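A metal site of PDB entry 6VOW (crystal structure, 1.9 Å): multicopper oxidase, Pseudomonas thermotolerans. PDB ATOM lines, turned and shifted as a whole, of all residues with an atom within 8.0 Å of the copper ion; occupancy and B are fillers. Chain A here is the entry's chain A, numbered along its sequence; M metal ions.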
ATOM      1  N   ALA A 191     -34.686  25.031  -5.809  1.00  0.00           N
ATOM      2  CA  ALA A 191     -33.510  25.883  -5.501  1.00  0.00           C
ATOM      3  C   ALA A 191     -33.686  26.593  -4.206  1.00  0.00           C
ATOM      4  O   ALA A 191     -32.707  26.796  -3.523  1.00  0.00           O
ATOM      5  CB  ALA A 191     -33.217  26.900  -6.626  1.00  0.00           C
ATOM      6  N   ARG A 193     -35.295  25.174  -1.742  1.00  0.00           N
ATOM      7  CA  ARG A 193     -35.231  24.046  -0.752  1.00  0.00           C
ATOM      8  C   ARG A 193     -33.839  23.351  -0.717  1.00  0.00           C
ATOM      9  O   ARG A 193     -32.837  24.019  -0.437  1.00  0.00           O
ATOM     10  CB  ARG A 193     -36.408  23.036  -0.874  1.00  0.00           C
ATOM     11  CG  ARG A 193     -36.772  22.453  -2.249  1.00  0.00           C
ATOM     12  CD  ARG A 193     -36.386  20.994  -2.654  1.00  0.00           C
ATOM     13  NE  ARG A 193     -37.286  19.903  -2.213  1.00  0.00           N
ATOM     14  CZ  ARG A 193     -38.515  19.615  -2.721  1.00  0.00           C
ATOM     15  NH1 ARG A 193     -39.076  20.342  -3.700  1.00  0.00           N
ATOM     16  NH2 ARG A 193     -39.208  18.585  -2.226  1.00  0.00           N
ATOM     17  N   GLU A 194     -33.781  22.036  -0.917  1.00  0.00           N
ATOM     18  CA  GLU A 194     -32.567  21.219  -0.772  1.00  0.00           C
ATOM     19  C   GLU A 194     -31.724  21.234  -2.052  1.00  0.00           C
ATOM     20  O   GLU A 194     -30.579  20.789  -2.062  1.00  0.00           O
ATOM     21  CB  GLU A 194     -32.957  19.783  -0.352  1.00  0.00           C
ATOM     22  CG  GLU A 194     -33.366  19.600   1.131  1.00  0.00           C
ATOM     23  CD  GLU A 194     -32.303  18.885   1.988  1.00  0.00           C
ATOM     24  OE1 GLU A 194     -31.933  17.737   1.626  1.00  0.00           O
ATOM     25  OE2 GLU A 194     -31.830  19.419   3.046  1.00  0.00           O
ATOM     26  N   GLY A 195     -32.316  21.787  -3.117  1.00  0.00           N
ATOM     27  CA  GLY A 195     -31.661  22.078  -4.373  1.00  0.00           C
ATOM     28  C   GLY A 195     -32.386  21.255  -5.394  1.00  0.00           C
ATOM     29  O   GLY A 195     -33.161  20.372  -5.029  1.00  0.00           O
ATOM     30  N   PHE A 329     -25.889  31.816   6.934  1.00  0.00           N
ATOM     31  CA  PHE A 329     -26.517  31.247   5.717  1.00  0.00           C
ATOM     32  C   PHE A 329     -28.016  31.021   6.058  1.00  0.00           C
ATOM     33  O   PHE A 329     -28.262  30.274   6.992  1.00  0.00           O
ATOM     34  CB  PHE A 329     -25.831  29.834   5.297  1.00  0.00           C
ATOM     35  CG  PHE A 329     -24.300  29.806   5.327  1.00  0.00           C
ATOM     36  CD1 PHE A 329     -23.552  29.902   4.138  1.00  0.00           C
ATOM     37  CD2 PHE A 329     -23.595  29.651   6.524  1.00  0.00           C
ATOM     38  CE1 PHE A 329     -22.148  29.908   4.144  1.00  0.00           C
ATOM     39  CE2 PHE A 329     -22.173  29.656   6.548  1.00  0.00           C
ATOM     40  CZ  PHE A 329     -21.465  29.767   5.352  1.00  0.00           C
ATOM     41  N   GLN A 349     -30.968  32.685  -1.591  1.00  0.00           N
ATOM     42  CA  GLN A 349     -30.052  32.481  -0.498  1.00  0.00           C
ATOM     43  C   GLN A 349     -29.118  33.677  -0.399  1.00  0.00           C
ATOM     44  O   GLN A 349     -28.854  34.354  -1.388  1.00  0.00           O
ATOM     45  CB  GLN A 349     -29.302  31.155  -0.697  1.00  0.00           C
ATOM     46  CG  GLN A 349     -30.216  29.984  -1.115  1.00  0.00           C
ATOM     47  CD  GLN A 349     -30.775  29.117   0.047  1.00  0.00           C
ATOM     48  OE1 GLN A 349     -30.521  29.338   1.284  1.00  0.00           O
ATOM     49  NE2 GLN A 349     -31.537  28.089  -0.335  1.00  0.00           N
ATOM     50  N   ASN A 382     -25.997  27.913   9.994  1.00  0.00           N
ATOM     51  CA  ASN A 382     -27.077  27.634   9.018  1.00  0.00           C
ATOM     52  C   ASN A 382     -28.344  28.094   9.732  1.00  0.00           C
ATOM     53  O   ASN A 382     -28.824  27.440  10.680  1.00  0.00           O
ATOM     54  CB  ASN A 382     -27.116  26.146   8.705  1.00  0.00           C
ATOM     55  CG  ASN A 382     -28.003  25.771   7.499  1.00  0.00           C
ATOM     56  OD1 ASN A 382     -28.647  26.588   6.872  1.00  0.00           O
ATOM     57  ND2 ASN A 382     -28.025  24.474   7.183  1.00  0.00           N
ATOM     58  N   TYR A 386     -32.364  23.658   5.940  1.00  0.00           N
ATOM     59  CA  TYR A 386     -31.829  23.111   4.720  1.00  0.00           C
ATOM     60  C   TYR A 386     -30.331  22.906   4.836  1.00  0.00           C
ATOM     61  O   TYR A 386     -29.626  23.786   5.328  1.00  0.00           O
ATOM     62  CB  TYR A 386     -32.256  24.033   3.610  1.00  0.00           C
ATOM     63  CG  TYR A 386     -33.753  23.885   3.419  1.00  0.00           C
ATOM     64  CD1 TYR A 386     -34.270  22.679   2.939  1.00  0.00           C
ATOM     65  CD2 TYR A 386     -34.649  24.882   3.783  1.00  0.00           C
ATOM     66  CE1 TYR A 386     -35.629  22.483   2.817  1.00  0.00           C
ATOM     67  CE2 TYR A 386     -36.008  24.699   3.661  1.00  0.00           C
ATOM     68  CZ  TYR A 386     -36.488  23.500   3.152  1.00  0.00           C
ATOM     69  OH  TYR A 386     -37.797  23.231   2.967  1.00  0.00           O
ATOM     70  N   GLN A 387     -29.838  21.711   4.511  1.00  0.00           N
ATOM     71  CA  GLN A 387     -28.373  21.493   4.693  1.00  0.00           C
ATOM     72  C   GLN A 387     -27.588  22.131   3.579  1.00  0.00           C
ATOM     73  O   GLN A 387     -28.074  22.235   2.451  1.00  0.00           O
ATOM     74  CB  GLN A 387     -27.977  20.046   4.887  1.00  0.00           C
ATOM     75  CG  GLN A 387     -28.134  19.070   3.735  1.00  0.00           C
ATOM     76  CD  GLN A 387     -28.086  17.646   4.266  1.00  0.00           C
ATOM     77  OE1 GLN A 387     -27.151  17.248   5.001  1.00  0.00           O
ATOM     78  NE2 GLN A 387     -29.149  16.889   3.966  1.00  0.00           N
ATOM     79  N   HIS A 388     -26.373  22.613   3.877  1.00  0.00           N
ATOM     80  CA  HIS A 388     -25.573  23.200   2.830  1.00  0.00           C
ATOM     81  C   HIS A 388     -24.160  22.603   2.884  1.00  0.00           C
ATOM     82  O   HIS A 388     -23.530  22.672   3.932  1.00  0.00           O
ATOM     83  CB  HIS A 388     -25.485  24.679   3.102  1.00  0.00           C
ATOM     84  CG  HIS A 388     -26.801  25.379   3.045  1.00  0.00           C
ATOM     85  ND1 HIS A 388     -27.626  25.325   1.954  1.00  0.00           N
ATOM     86  CD2 HIS A 388     -27.435  26.139   3.967  1.00  0.00           C
ATOM     87  CE1 HIS A 388     -28.724  26.027   2.197  1.00  0.00           C
ATOM     88  NE2 HIS A 388     -28.617  26.551   3.409  1.00  0.00           N
ATOM     89  N   PRO A 389     -23.642  22.005   1.798  1.00  0.00           N
ATOM     90  CA  PRO A 389     -22.199  21.585   1.780  1.00  0.00           C
ATOM     91  C   PRO A 389     -21.334  22.797   1.441  1.00  0.00           C
ATOM     92  O   PRO A 389     -21.247  23.263   0.266  1.00  0.00           O
ATOM     93  CB  PRO A 389     -22.154  20.530   0.680  1.00  0.00           C
ATOM     94  CG  PRO A 389     -23.219  21.035  -0.266  1.00  0.00           C
ATOM     95  CD  PRO A 389     -24.333  21.445   0.649  1.00  0.00           C
ATOM     96  N   ILE A 390     -20.779  23.356   2.500  1.00  0.00           N
ATOM     97  CA  ILE A 390     -20.178  24.631   2.385  1.00  0.00           C
ATOM     98  C   ILE A 390     -18.752  24.421   2.070  1.00  0.00           C
ATOM     99  O   ILE A 390     -18.009  23.782   2.860  1.00  0.00           O
ATOM    100  CB  ILE A 390     -20.254  25.416   3.650  1.00  0.00           C
ATOM    101  CG1 ILE A 390     -21.751  25.691   4.031  1.00  0.00           C
ATOM    102  CG2 ILE A 390     -19.429  26.704   3.484  1.00  0.00           C
ATOM    103  CD1 ILE A 390     -22.460  26.747   3.257  1.00  0.00           C
ATOM    104  N   LEU A 416     -20.451  19.799   5.537  1.00  0.00           N
ATOM    105  CA  LEU A 416     -21.897  19.636   5.284  1.00  0.00           C
ATOM    106  C   LEU A 416     -22.675  20.206   6.502  1.00  0.00           C
ATOM    107  O   LEU A 416     -22.805  19.580   7.602  1.00  0.00           O
ATOM    108  CB  LEU A 416     -22.228  18.152   4.952  1.00  0.00           C
ATOM    109  CG  LEU A 416     -23.635  17.756   4.554  1.00  0.00           C
ATOM    110  CD1 LEU A 416     -24.159  18.493   3.330  1.00  0.00           C
ATOM    111  CD2 LEU A 416     -23.693  16.268   4.338  1.00  0.00           C
ATOM    112  N   LEU A 417     -23.158  21.416   6.289  1.00  0.00           N
ATOM    113  CA  LEU A 417     -23.721  22.221   7.333  1.00  0.00           C
ATOM    114  C   LEU A 417     -25.178  21.925   7.494  1.00  0.00           C
ATOM    115  O   LEU A 417     -26.001  22.299   6.643  1.00  0.00           O
ATOM    116  CB  LEU A 417     -23.538  23.677   6.989  1.00  0.00           C
ATOM    117  CG  LEU A 417     -23.775  24.610   8.167  1.00  0.00           C
ATOM    118  CD1 LEU A 417     -22.839  24.327   9.299  1.00  0.00           C
ATOM    119  CD2 LEU A 417     -23.578  26.054   7.639  1.00  0.00           C
ATOM    120  N   HIS A 438     -18.744  29.026  -0.854  1.00  0.00           N
ATOM    121  CA  HIS A 438     -20.081  28.791  -1.317  1.00  0.00           C
ATOM    122  C   HIS A 438     -20.660  27.399  -0.968  1.00  0.00           C
ATOM    123  O   HIS A 438     -19.945  26.399  -0.646  1.00  0.00           O
ATOM    124  CB  HIS A 438     -20.164  29.119  -2.806  1.00  0.00           C
ATOM    125  CG  HIS A 438     -19.515  28.074  -3.655  1.00  0.00           C
ATOM    126  ND1 HIS A 438     -20.136  26.898  -3.953  1.00  0.00           N
ATOM    127  CD2 HIS A 438     -18.264  27.979  -4.153  1.00  0.00           C
ATOM    128  CE1 HIS A 438     -19.340  26.143  -4.657  1.00  0.00           C
ATOM    129  NE2 HIS A 438     -18.201  26.775  -4.790  1.00  0.00           N
ATOM    130  N   CYS A 439     -21.995  27.328  -1.027  1.00  0.00           N
ATOM    131  CA  CYS A 439     -22.648  26.068  -0.850  1.00  0.00           C
ATOM    132  C   CYS A 439     -22.390  25.348  -2.152  1.00  0.00           C
ATOM    133  O   CYS A 439     -22.444  25.960  -3.251  1.00  0.00           O
ATOM    134  CB  CYS A 439     -24.150  26.197  -0.636  1.00  0.00           C
ATOM    135  SG  CYS A 439     -24.955  24.580  -0.807  1.00  0.00           S
ATOM    136  N   HIS A 440     -22.092  24.055  -2.054  1.00  0.00           N
ATOM    137  CA  HIS A 440     -21.782  23.254  -3.268  1.00  0.00           C
ATOM    138  C   HIS A 440     -23.009  22.493  -3.887  1.00  0.00           C
ATOM    139  O   HIS A 440     -22.871  21.573  -4.752  1.00  0.00           O
ATOM    140  CB  HIS A 440     -20.574  22.378  -2.996  1.00  0.00           C
ATOM    141  CG  HIS A 440     -19.671  22.249  -4.193  1.00  0.00           C
ATOM    142  ND1 HIS A 440     -20.057  21.536  -5.315  1.00  0.00           N
ATOM    143  CD2 HIS A 440     -18.472  22.818  -4.495  1.00  0.00           C
ATOM    144  CE1 HIS A 440     -19.115  21.663  -6.237  1.00  0.00           C
ATOM    145  NE2 HIS A 440     -18.137  22.413  -5.759  1.00  0.00           N
ATOM    146  N   VAL A 441     -24.216  22.899  -3.450  1.00  0.00           N
ATOM    147  CA  VAL A 441     -25.466  22.493  -4.085  1.00  0.00           C
ATOM    148  C   VAL A 441     -25.520  23.592  -5.087  1.00  0.00           C
ATOM    149  O   VAL A 441     -25.563  24.805  -4.713  1.00  0.00           O
ATOM    150  CB  VAL A 441     -26.675  22.517  -3.126  1.00  0.00           C
ATOM    151  CG1 VAL A 441     -27.971  22.404  -3.889  1.00  0.00           C
ATOM    152  CG2 VAL A 441     -26.610  21.333  -2.150  1.00  0.00           C
ATOM    153  N   ILE A 442     -25.378  23.187  -6.352  1.00  0.00           N
ATOM    154  CA  ILE A 442     -25.038  24.138  -7.418  1.00  0.00           C
ATOM    155  C   ILE A 442     -26.131  25.185  -7.617  1.00  0.00           C
ATOM    156  O   ILE A 442     -25.852  26.352  -7.829  1.00  0.00           O
ATOM    157  CB  ILE A 442     -24.719  23.444  -8.766  1.00  0.00           C
ATOM    158  CG1 ILE A 442     -23.616  22.362  -8.630  1.00  0.00           C
ATOM    159  CG2 ILE A 442     -24.368  24.508  -9.814  1.00  0.00           C
ATOM    160  CD1 ILE A 442     -22.263  22.908  -8.132  1.00  0.00           C
ATOM    161  N   ASP A 443     -27.368  24.768  -7.515  1.00  0.00           N
ATOM    162  CA  ASP A 443     -28.540  25.672  -7.327  1.00  0.00           C
ATOM    163  C   ASP A 443     -28.464  26.730  -6.269  1.00  0.00           C
ATOM    164  O   ASP A 443     -28.832  27.850  -6.518  1.00  0.00           O
ATOM    165  CB  ASP A 443     -29.739  24.825  -6.919  1.00  0.00           C
ATOM    166  CG  ASP A 443     -30.518  24.437  -8.055  1.00  0.00           C
ATOM    167  OD1 ASP A 443     -30.026  24.520  -9.185  1.00  0.00           O
ATOM    168  OD2 ASP A 443     -31.675  24.073  -7.823  1.00  0.00           O
ATOM    169  N   HIS A 444     -28.049  26.387  -5.085  1.00  0.00           N
ATOM    170  CA  HIS A 444     -27.940  27.387  -4.050  1.00  0.00           C
ATOM    171  C   HIS A 444     -26.843  28.342  -4.325  1.00  0.00           C
ATOM    172  O   HIS A 444     -27.004  29.504  -3.987  1.00  0.00           O
ATOM    173  CB  HIS A 444     -27.659  26.785  -2.698  1.00  0.00           C
ATOM    174  CG  HIS A 444     -28.777  25.990  -2.174  1.00  0.00           C
ATOM    175  ND1 HIS A 444     -28.679  25.305  -0.995  1.00  0.00           N
ATOM    176  CD2 HIS A 444     -30.016  25.724  -2.676  1.00  0.00           C
ATOM    177  CE1 HIS A 444     -29.817  24.685  -0.761  1.00  0.00           C
ATOM    178  NE2 HIS A 444     -30.637  24.913  -1.763  1.00  0.00           N
ATOM    179  N   MET A 445     -25.725  27.850  -4.902  1.00  0.00           N
ATOM    180  CA  MET A 445     -24.593  28.683  -5.222  1.00  0.00           C
ATOM    181  C   MET A 445     -25.050  29.656  -6.272  1.00  0.00           C
ATOM    182  O   MET A 445     -24.777  30.840  -6.177  1.00  0.00           O
ATOM    183  CB  MET A 445     -23.423  27.863  -5.762  1.00  0.00           C
ATOM    184  CG  MET A 445     -22.275  28.658  -6.396  1.00  0.00           C
ATOM    185  SD  MET A 445     -21.138  27.539  -7.254  1.00  0.00           S
ATOM    186  CE  MET A 445     -22.032  27.515  -8.783  1.00  0.00           C
ATOM    187  N   THR A 447     -28.103  30.653  -6.886  1.00  0.00           N
ATOM    188  CA  THR A 447     -29.222  31.509  -6.501  1.00  0.00           C
ATOM    189  C   THR A 447     -28.832  32.277  -5.277  1.00  0.00           C
ATOM    190  O   THR A 447     -29.697  32.573  -4.467  1.00  0.00           O
ATOM    191  CB  THR A 447     -30.540  30.712  -6.317  1.00  0.00           C
ATOM    192  OG1 THR A 447     -30.439  29.703  -5.283  1.00  0.00           O
ATOM    193  CG2 THR A 447     -30.897  30.085  -7.633  1.00  0.00           C
ATOM    194  N   LEU A 449     -25.961  31.720  -2.745  1.00  0.00           N
ATOM    195  CA  LEU A 449     -25.212  31.245  -1.578  1.00  0.00           C
ATOM    196  C   LEU A 449     -23.718  31.118  -1.909  1.00  0.00           C
ATOM    197  O   LEU A 449     -23.145  30.029  -1.988  1.00  0.00           O
ATOM    198  CB  LEU A 449     -25.812  29.930  -1.096  1.00  0.00           C
ATOM    199  CG  LEU A 449     -25.548  29.483   0.325  1.00  0.00           C
ATOM    200  CD1 LEU A 449     -25.818  30.625   1.289  1.00  0.00           C
ATOM    201  CD2 LEU A 449     -26.428  28.265   0.639  1.00  0.00           C
HETATM  202 CU    CU M   1     -26.938  25.015   0.081  1.00  0.00          CU
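The backbone carbonyl oxygen (O) of His 388 sits at hydrogen-bond distance from the backbone NH (N) of Leu 417 (2.7 Å). A ring nitrogen (NE2) of His 388 lies close to the side-chain amide oxygen (OD1) of Asn 382, 3.5 Å away. The backbone carbonyl oxygen of His 444 is in hydrogen-bond range of the backbone NH of Leu 449 (2.7 Å). A ring nitrogen (NE2) of His 444 lies within hydrogen-bond range of the backbone carbonyl oxygen (O) of Arg 193, at 2.7 Å. NE2 of His 444 lies close to O of Ala 191, 3.3 Å away. N of Cys 439 is in hydrogen-bond range of O of Leu 449 (3.1 Å). The backbone NH of Val 441 lies close to the side-chain sulfur of Cys 439. OE2 of Glu 194 sits at hydrogen-bond distance from N of Gln 387 (3.4 Å).
Gln 387 touches the copper ion (O to CU, 3.8 Å). Leu 449 touches the copper ion (CD2 to CU, 3.3 Å). Along chain A the residues within 4 Å of the copper ion span positions 387 to 449.
The copper ion is bound by ND1 of His 388 (2.0 Å), ND1 of His 444 (2.1 Å) and SG of Cys 439 (2.2 Å).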
